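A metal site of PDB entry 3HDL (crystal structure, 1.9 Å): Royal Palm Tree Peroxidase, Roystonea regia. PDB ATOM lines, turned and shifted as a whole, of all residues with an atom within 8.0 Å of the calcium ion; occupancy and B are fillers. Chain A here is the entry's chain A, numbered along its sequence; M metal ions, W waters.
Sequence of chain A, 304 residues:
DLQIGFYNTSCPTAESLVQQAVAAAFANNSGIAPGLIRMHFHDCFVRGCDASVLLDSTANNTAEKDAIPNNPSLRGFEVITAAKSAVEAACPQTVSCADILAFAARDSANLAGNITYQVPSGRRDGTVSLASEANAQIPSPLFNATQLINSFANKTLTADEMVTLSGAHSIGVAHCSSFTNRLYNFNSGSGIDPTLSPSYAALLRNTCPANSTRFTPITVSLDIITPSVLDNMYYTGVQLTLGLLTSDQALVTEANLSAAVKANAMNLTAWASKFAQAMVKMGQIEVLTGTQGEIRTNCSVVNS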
ATOM      1  N   MET A  39     -19.142  -9.234   8.379  1.00  0.00           N
ATOM      2  CA  MET A  39     -18.579  -9.564   7.076  1.00  0.00           C
ATOM      3  C   MET A  39     -17.257  -8.826   6.837  1.00  0.00           C
ATOM      4  O   MET A  39     -16.321  -9.410   6.308  1.00  0.00           O
ATOM      5  CB  MET A  39     -19.573  -9.275   5.957  1.00  0.00           C
ATOM      6  CG  MET A  39     -19.139  -9.813   4.609  1.00  0.00           C
ATOM      7  SD  MET A  39     -20.409  -9.592   3.349  1.00  0.00           S
ATOM      8  CE  MET A  39     -21.707 -10.638   4.007  1.00  0.00           C
ATOM      9  N   HIS A  40     -17.209  -7.552   7.211  1.00  0.00           N
ATOM     10  CA  HIS A  40     -15.996  -6.759   7.050  1.00  0.00           C
ATOM     11  C   HIS A  40     -14.874  -7.321   7.925  1.00  0.00           C
ATOM     12  O   HIS A  40     -13.732  -7.434   7.489  1.00  0.00           O
ATOM     13  CB  HIS A  40     -16.252  -5.275   7.372  1.00  0.00           C
ATOM     14  CG  HIS A  40     -15.074  -4.381   7.113  1.00  0.00           C
ATOM     15  ND1 HIS A  40     -14.665  -3.418   8.006  1.00  0.00           N
ATOM     16  CD2 HIS A  40     -14.232  -4.305   6.065  1.00  0.00           C
ATOM     17  CE1 HIS A  40     -13.616  -2.781   7.523  1.00  0.00           C
ATOM     18  NE2 HIS A  40     -13.330  -3.299   6.336  1.00  0.00           N
ATOM     19  N   PHE A  41     -15.219  -7.697   9.149  1.00  0.00           N
ATOM     20  CA  PHE A  41     -14.268  -8.379  10.054  1.00  0.00           C
ATOM     21  C   PHE A  41     -13.720  -9.644   9.377  1.00  0.00           C
ATOM     22  O   PHE A  41     -12.494  -9.842   9.326  1.00  0.00           O
ATOM     23  CB  PHE A  41     -14.986  -8.690  11.382  1.00  0.00           C
ATOM     24  CG  PHE A  41     -14.251  -9.659  12.280  1.00  0.00           C
ATOM     25  CD1 PHE A  41     -12.882  -9.555  12.480  1.00  0.00           C
ATOM     26  CD2 PHE A  41     -14.944 -10.648  12.963  1.00  0.00           C
ATOM     27  CE1 PHE A  41     -12.216 -10.433  13.322  1.00  0.00           C
ATOM     28  CE2 PHE A  41     -14.294 -11.531  13.800  1.00  0.00           C
ATOM     29  CZ  PHE A  41     -12.921 -11.427  13.986  1.00  0.00           C
ATOM     30  N   HIS A  42     -14.599 -10.473   8.840  1.00  0.00           N
ATOM     31  CA  HIS A  42     -14.170 -11.722   8.209  1.00  0.00           C
ATOM     32  C   HIS A  42     -13.358 -11.468   6.946  1.00  0.00           C
ATOM     33  O   HIS A  42     -12.491 -12.271   6.587  1.00  0.00           O
ATOM     34  CB  HIS A  42     -15.381 -12.623   7.935  1.00  0.00           C
ATOM     35  CG  HIS A  42     -15.897 -13.310   9.158  1.00  0.00           C
ATOM     36  ND1 HIS A  42     -16.400 -14.596   9.136  1.00  0.00           N
ATOM     37  CD2 HIS A  42     -15.950 -12.907  10.450  1.00  0.00           C
ATOM     38  CE1 HIS A  42     -16.759 -14.943  10.356  1.00  0.00           C
ATOM     39  NE2 HIS A  42     -16.497 -13.944  11.175  1.00  0.00           N
ATOM     40  N   ASP A  43     -13.622 -10.360   6.261  1.00  0.00           N
ATOM     41  CA  ASP A  43     -12.769  -9.965   5.151  1.00  0.00           C
ATOM     42  C   ASP A  43     -11.379  -9.665   5.682  1.00  0.00           C
ATOM     43  O   ASP A  43     -10.399 -10.257   5.247  1.00  0.00           O
ATOM     44  CB  ASP A  43     -13.336  -8.740   4.429  1.00  0.00           C
ATOM     45  CG  ASP A  43     -12.614  -8.464   3.125  1.00  0.00           C
ATOM     46  OD1 ASP A  43     -11.901  -9.369   2.653  1.00  0.00           O
ATOM     47  OD2 ASP A  43     -12.747  -7.346   2.560  1.00  0.00           O
ATOM     48  N   CYS A  44     -11.283  -8.771   6.644  1.00  0.00           N
ATOM     49  CA  CYS A  44      -9.985  -8.287   7.097  1.00  0.00           C
ATOM     50  C   CYS A  44      -9.095  -9.350   7.746  1.00  0.00           C
ATOM     51  O   CYS A  44      -7.863  -9.214   7.736  1.00  0.00           O
ATOM     52  CB  CYS A  44     -10.161  -7.087   8.031  1.00  0.00           C
ATOM     53  SG  CYS A  44     -10.978  -5.701   7.213  1.00  0.00           S
ATOM     54  N   PHE A  45      -9.701 -10.387   8.314  1.00  0.00           N
ATOM     55  CA  PHE A  45      -8.928 -11.422   8.988  1.00  0.00           C
ATOM     56  C   PHE A  45      -8.442 -12.566   8.094  1.00  0.00           C
ATOM     57  O   PHE A  45      -7.771 -13.490   8.569  1.00  0.00           O
ATOM     58  CB  PHE A  45      -9.700 -11.978  10.188  1.00  0.00           C
ATOM     59  CG  PHE A  45      -9.297 -11.380  11.497  1.00  0.00           C
ATOM     60  CD1 PHE A  45      -9.193 -10.005  11.638  1.00  0.00           C
ATOM     61  CD2 PHE A  45      -9.013 -12.183  12.588  1.00  0.00           C
ATOM     62  CE1 PHE A  45      -8.811  -9.439  12.837  1.00  0.00           C
ATOM     63  CE2 PHE A  45      -8.637 -11.623  13.793  1.00  0.00           C
ATOM     64  CZ  PHE A  45      -8.534 -10.253  13.926  1.00  0.00           C
ATOM     65  N   VAL A  46      -8.771 -12.526   6.810  1.00  0.00           N
ATOM     66  CA  VAL A  46      -8.236 -13.520   5.887  1.00  0.00           C
ATOM     67  C   VAL A  46      -7.648 -12.841   4.663  1.00  0.00           C
ATOM     68  O   VAL A  46      -8.379 -12.313   3.844  1.00  0.00           O
ATOM     69  CB  VAL A  46      -9.308 -14.551   5.454  1.00  0.00           C
ATOM     70  CG1 VAL A  46      -8.665 -15.750   4.769  1.00  0.00           C
ATOM     71  CG2 VAL A  46     -10.152 -14.988   6.640  1.00  0.00           C
ATOM     72  N   ARG A  47      -6.326 -12.851   4.531  1.00  0.00           N
ATOM     73  CA  ARG A  47      -5.678 -12.176   3.406  1.00  0.00           C
ATOM     74  C   ARG A  47      -5.973 -10.673   3.377  1.00  0.00           C
ATOM     75  O   ARG A  47      -5.948 -10.067   2.303  1.00  0.00           O
ATOM     76  CB  ARG A  47      -6.137 -12.772   2.072  1.00  0.00           C
ATOM     77  CG  ARG A  47      -5.855 -14.243   1.920  1.00  0.00           C
ATOM     78  CD  ARG A  47      -6.174 -14.692   0.511  1.00  0.00           C
ATOM     79  NE  ARG A  47      -5.328 -15.806   0.137  1.00  0.00           N
ATOM     80  CZ  ARG A  47      -4.240 -15.693  -0.617  1.00  0.00           C
ATOM     81  NH1 ARG A  47      -3.873 -14.509  -1.086  1.00  0.00           N
ATOM     82  NH2 ARG A  47      -3.517 -16.762  -0.902  1.00  0.00           N
ATOM     83  N   GLY A  48      -6.280 -10.096   4.528  1.00  0.00           N
ATOM     84  CA  GLY A  48      -6.490  -8.656   4.620  1.00  0.00           C
ATOM     85  C   GLY A  48      -7.807  -8.207   4.011  1.00  0.00           C
ATOM     86  O   GLY A  48      -8.526  -9.013   3.440  1.00  0.00           O
ATOM     87  N   CYS A  49      -8.116  -6.926   4.139  1.00  0.00           N
ATOM     88  CA  CYS A  49      -9.385  -6.388   3.655  1.00  0.00           C
ATOM     89  C   CYS A  49      -9.359  -6.237   2.137  1.00  0.00           C
ATOM     90  O   CYS A  49      -9.140  -5.139   1.617  1.00  0.00           O
ATOM     91  CB  CYS A  49      -9.671  -5.029   4.322  1.00  0.00           C
ATOM     92  SG  CYS A  49      -9.387  -5.001   6.132  1.00  0.00           S
ATOM     93  N   ASP A  50      -9.570  -7.344   1.428  1.00  0.00           N
ATOM     94  CA  ASP A  50      -9.397  -7.396  -0.026  1.00  0.00           C
ATOM     95  C   ASP A  50     -10.620  -7.989  -0.722  1.00  0.00           C
ATOM     96  O   ASP A  50     -10.519  -8.442  -1.867  1.00  0.00           O
ATOM     97  CB  ASP A  50      -8.169  -8.242  -0.389  1.00  0.00           C
ATOM     98  CG  ASP A  50      -8.392  -9.723  -0.100  1.00  0.00           C
ATOM     99  OD1 ASP A  50      -9.320 -10.017   0.686  1.00  0.00           O
ATOM    100  OD2 ASP A  50      -7.673 -10.580  -0.644  1.00  0.00           O
ATOM    101  N   ALA A  51     -11.755  -8.002  -0.026  1.00  0.00           N
ATOM    102  CA  ALA A  51     -13.005  -8.527  -0.575  1.00  0.00           C
ATOM    103  C   ALA A  51     -12.971 -10.007  -0.941  1.00  0.00           C
ATOM    104  O   ALA A  51     -13.850 -10.504  -1.646  1.00  0.00           O
ATOM    105  CB  ALA A  51     -13.463  -7.686  -1.784  1.00  0.00           C
ATOM    106  N   SER A  52     -11.967 -10.737  -0.441  1.00  0.00           N
ATOM    107  CA  SER A  52     -11.888 -12.157  -0.748  1.00  0.00           C
ATOM    108  C   SER A  52     -13.117 -12.926  -0.238  1.00  0.00           C
ATOM    109  O   SER A  52     -13.575 -13.873  -0.880  1.00  0.00           O
ATOM    110  CB  SER A  52     -10.595 -12.766  -0.184  1.00  0.00           C
ATOM    111  OG  SER A  52     -10.613 -12.783   1.227  1.00  0.00           O
ATOM    112  N   VAL A  53     -13.661 -12.489   0.886  1.00  0.00           N
ATOM    113  CA  VAL A  53     -14.820 -13.152   1.491  1.00  0.00           C
ATOM    114  C   VAL A  53     -16.061 -13.123   0.593  1.00  0.00           C
ATOM    115  O   VAL A  53     -16.960 -13.951   0.758  1.00  0.00           O
ATOM    116  CB  VAL A  53     -15.166 -12.514   2.859  1.00  0.00           C
ATOM    117  CG1 VAL A  53     -15.746 -11.129   2.665  1.00  0.00           C
ATOM    118  CG2 VAL A  53     -16.139 -13.407   3.636  1.00  0.00           C
ATOM    119  N   LEU A  54     -16.100 -12.187  -0.343  1.00  0.00           N
ATOM    120  CA  LEU A  54     -17.281 -11.999  -1.194  1.00  0.00           C
ATOM    121  C   LEU A  54     -17.373 -12.982  -2.369  1.00  0.00           C
ATOM    122  O   LEU A  54     -18.429 -13.126  -2.984  1.00  0.00           O
ATOM    123  CB  LEU A  54     -17.328 -10.567  -1.725  1.00  0.00           C
ATOM    124  CG  LEU A  54     -17.412  -9.448  -0.697  1.00  0.00           C
ATOM    125  CD1 LEU A  54     -17.383  -8.091  -1.383  1.00  0.00           C
ATOM    126  CD2 LEU A  54     -18.678  -9.602   0.144  1.00  0.00           C
ATOM    127  N   GLU A  64     -14.041 -18.878   0.619  1.00  0.00           N
ATOM    128  CA  GLU A  64     -14.213 -18.594   2.036  1.00  0.00           C
ATOM    129  C   GLU A  64     -15.672 -18.728   2.467  1.00  0.00           C
ATOM    130  O   GLU A  64     -15.952 -19.140   3.599  1.00  0.00           O
ATOM    131  CB  GLU A  64     -13.700 -17.187   2.357  1.00  0.00           C
ATOM    132  CG  GLU A  64     -12.202 -17.012   2.175  1.00  0.00           C
ATOM    133  CD  GLU A  64     -11.744 -15.602   2.508  1.00  0.00           C
ATOM    134  OE1 GLU A  64     -12.476 -14.892   3.232  1.00  0.00           O
ATOM    135  OE2 GLU A  64     -10.655 -15.204   2.043  1.00  0.00           O
ATOM    136  N   ALA A  98     -13.822  -4.172  -1.955  1.00  0.00           N
ATOM    137  CA  ALA A  98     -13.216  -4.097  -0.624  1.00  0.00           C
ATOM    138  C   ALA A  98     -13.562  -2.788   0.068  1.00  0.00           C
ATOM    139  O   ALA A  98     -13.894  -2.783   1.261  1.00  0.00           O
ATOM    140  CB  ALA A  98     -11.695  -4.271  -0.721  1.00  0.00           C
ATOM    141  N   LEU A 101     -17.340  -2.707   1.052  1.00  0.00           N
ATOM    142  CA  LEU A 101     -17.596  -3.462   2.278  1.00  0.00           C
ATOM    143  C   LEU A 101     -17.183  -2.667   3.510  1.00  0.00           C
ATOM    144  O   LEU A 101     -17.892  -2.655   4.524  1.00  0.00           O
ATOM    145  CB  LEU A 101     -16.891  -4.813   2.229  1.00  0.00           C
ATOM    146  CG  LEU A 101     -17.035  -5.723   3.458  1.00  0.00           C
ATOM    147  CD1 LEU A 101     -18.510  -5.942   3.802  1.00  0.00           C
ATOM    148  CD2 LEU A 101     -16.342  -7.046   3.207  1.00  0.00           C
ATOM    149  N   GLY A 126      -8.751  -8.590  -4.176  1.00  0.00           N
ATOM    150  CA  GLY A 126      -7.903  -9.747  -4.410  1.00  0.00           C
ATOM    151  C   GLY A 126      -8.573 -10.763  -5.321  1.00  0.00           C
ATOM    152  O   GLY A 126      -9.734 -10.607  -5.693  1.00  0.00           O
ATOM    153  N   VAL A 128      -8.080 -14.316  -4.771  1.00  0.00           N
ATOM    154  CA  VAL A 128      -7.996 -15.608  -4.111  1.00  0.00           C
ATOM    155  C   VAL A 128      -9.002 -15.685  -2.956  1.00  0.00           C
ATOM    156  O   VAL A 128      -9.174 -14.714  -2.213  1.00  0.00           O
ATOM    157  CB  VAL A 128      -6.583 -15.875  -3.553  1.00  0.00           C
ATOM    158  CG1 VAL A 128      -6.579 -17.149  -2.710  1.00  0.00           C
ATOM    159  CG2 VAL A 128      -5.565 -15.972  -4.691  1.00  0.00           C
ATOM    160  N   SER A 129      -9.658 -16.828  -2.824  1.00  0.00           N
ATOM    161  CA  SER A 129     -10.577 -17.059  -1.710  1.00  0.00           C
ATOM    162  C   SER A 129     -10.689 -18.544  -1.411  1.00  0.00           C
ATOM    163  O   SER A 129     -11.166 -19.309  -2.249  1.00  0.00           O
ATOM    164  CB  SER A 129     -11.962 -16.485  -2.014  1.00  0.00           C
ATOM    165  OG  SER A 129     -12.843 -16.710  -0.927  1.00  0.00           O
ATOM    166  N   GLU A 133      -8.479 -21.326   4.311  1.00  0.00           N
ATOM    167  CA  GLU A 133      -7.875 -20.182   4.989  1.00  0.00           C
ATOM    168  C   GLU A 133      -8.825 -19.543   5.994  1.00  0.00           C
ATOM    169  O   GLU A 133      -8.408 -19.179   7.100  1.00  0.00           O
ATOM    170  CB  GLU A 133      -7.378 -19.151   3.969  1.00  0.00           C
ATOM    171  CG  GLU A 133      -6.171 -19.631   3.159  1.00  0.00           C
ATOM    172  CD  GLU A 133      -5.615 -18.574   2.229  1.00  0.00           C
ATOM    173  OE1 GLU A 133      -6.208 -17.480   2.140  1.00  0.00           O
ATOM    174  OE2 GLU A 133      -4.587 -18.841   1.581  1.00  0.00           O
ATOM    175  N   ILE A 285      -5.910  -3.775   7.572  1.00  0.00           N
ATOM    176  CA  ILE A 285      -5.101  -4.982   7.695  1.00  0.00           C
ATOM    177  C   ILE A 285      -4.760  -5.563   6.326  1.00  0.00           C
ATOM    178  O   ILE A 285      -5.652  -5.908   5.544  1.00  0.00           O
ATOM    179  CB  ILE A 285      -5.823  -6.060   8.546  1.00  0.00           C
ATOM    180  CG1 ILE A 285      -5.961  -5.593   9.990  1.00  0.00           C
ATOM    181  CG2 ILE A 285      -5.071  -7.389   8.482  1.00  0.00           C
ATOM    182  CD1 ILE A 285      -6.912  -6.441  10.818  1.00  0.00           C
ATOM    183  N   GLU A 286      -3.462  -5.639   6.046  1.00  0.00           N
ATOM    184  CA  GLU A 286      -2.956  -6.286   4.829  1.00  0.00           C
ATOM    185  C   GLU A 286      -3.708  -5.900   3.553  1.00  0.00           C
ATOM    186  O   GLU A 286      -4.063  -6.763   2.751  1.00  0.00           O
ATOM    187  CB  GLU A 286      -2.963  -7.803   4.997  1.00  0.00           C
ATOM    188  CG  GLU A 286      -2.325  -8.288   6.297  1.00  0.00           C
ATOM    189  CD  GLU A 286      -2.452  -9.789   6.473  1.00  0.00           C
ATOM    190  OE1 GLU A 286      -3.002 -10.223   7.518  1.00  0.00           O
ATOM    191  OE2 GLU A 286      -2.025 -10.531   5.579  1.00  0.00           O
ATOM    192  N   ARG A 296     -12.818  -5.259  -8.926  1.00  0.00           N
ATOM    193  CA  ARG A 296     -13.757  -6.309  -9.283  1.00  0.00           C
ATOM    194  C   ARG A 296     -15.069  -5.660  -9.720  1.00  0.00           C
ATOM    195  O   ARG A 296     -15.589  -4.807  -9.014  1.00  0.00           O
ATOM    196  CB  ARG A 296     -13.971  -7.216  -8.075  1.00  0.00           C
ATOM    197  CG  ARG A 296     -14.484  -8.606  -8.395  1.00  0.00           C
ATOM    198  CD  ARG A 296     -14.731  -9.392  -7.101  1.00  0.00           C
ATOM    199  NE  ARG A 296     -13.501  -9.672  -6.361  1.00  0.00           N
ATOM    200  CZ  ARG A 296     -13.467  -9.961  -5.062  1.00  0.00           C
ATOM    201  NH1 ARG A 296     -14.595  -9.979  -4.364  1.00  0.00           N
ATOM    202  NH2 ARG A 296     -12.311 -10.201  -4.456  1.00  0.00           N
HETATM  203 CA    CA M   1     -10.044 -10.949   2.893  1.00  0.00          CA
HETATM  204  O   HOH W   1     -11.688 -12.624   3.992  1.00  0.00           O
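Water W1 bridges the side-chain carboxylate of Glu 64 and the backbone carbonyl oxygen of His 42.
The backbone carbonyl oxygen (O) of Ser 52 sits at hydrogen-bond distance from the side-chain hydroxyl (OG) of Ser 129 (2.9 Å). The backbone NH (N) of Ala 51 sits at hydrogen-bond distance from the side-chain carboxylate (OD2) of Asp 43 (2.8 Å). The backbone carbonyl oxygen (O) of Asp 50 lies within hydrogen-bond range of the backbone NH (N) of Gly 126 (2.9 Å). The side-chain sulfur (SG) of Cys 49 forms a disulfide with the side-chain sulfur (SG) of Cys 44 (2.0 Å). OG of Ser 52 lies close to OE2 of Glu 64.
Five residues have an atom within 4 Å of the calcium ion: Asp 43, Val 46, Gly 48, Asp 50 and Ser 52. The nearest printed residue that does not touch the calcium ion is Arg 47 (4.1 Å).
The calcium ion is bound by the backbone carbonyl oxygen (O) of Val 46, at 2.4 Å. OD1 of Asp 43 is bound to the calcium ion. The calcium ion is bound by the backbone carbonyl oxygen (O) of Asp 43 (2.5 Å). The side-chain carboxylate (OD1) of Asp 50 is bound to the calcium ion, at 2.5 Å. The calcium ion is bound by O of Gly 48 (2.5 Å). OG of Ser 52 is bound to the calcium ion, 2.5 Å away. Water W1 is bound to the calcium ion (2.6 Å). The calcium ion has seven donor atoms within binding distance.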
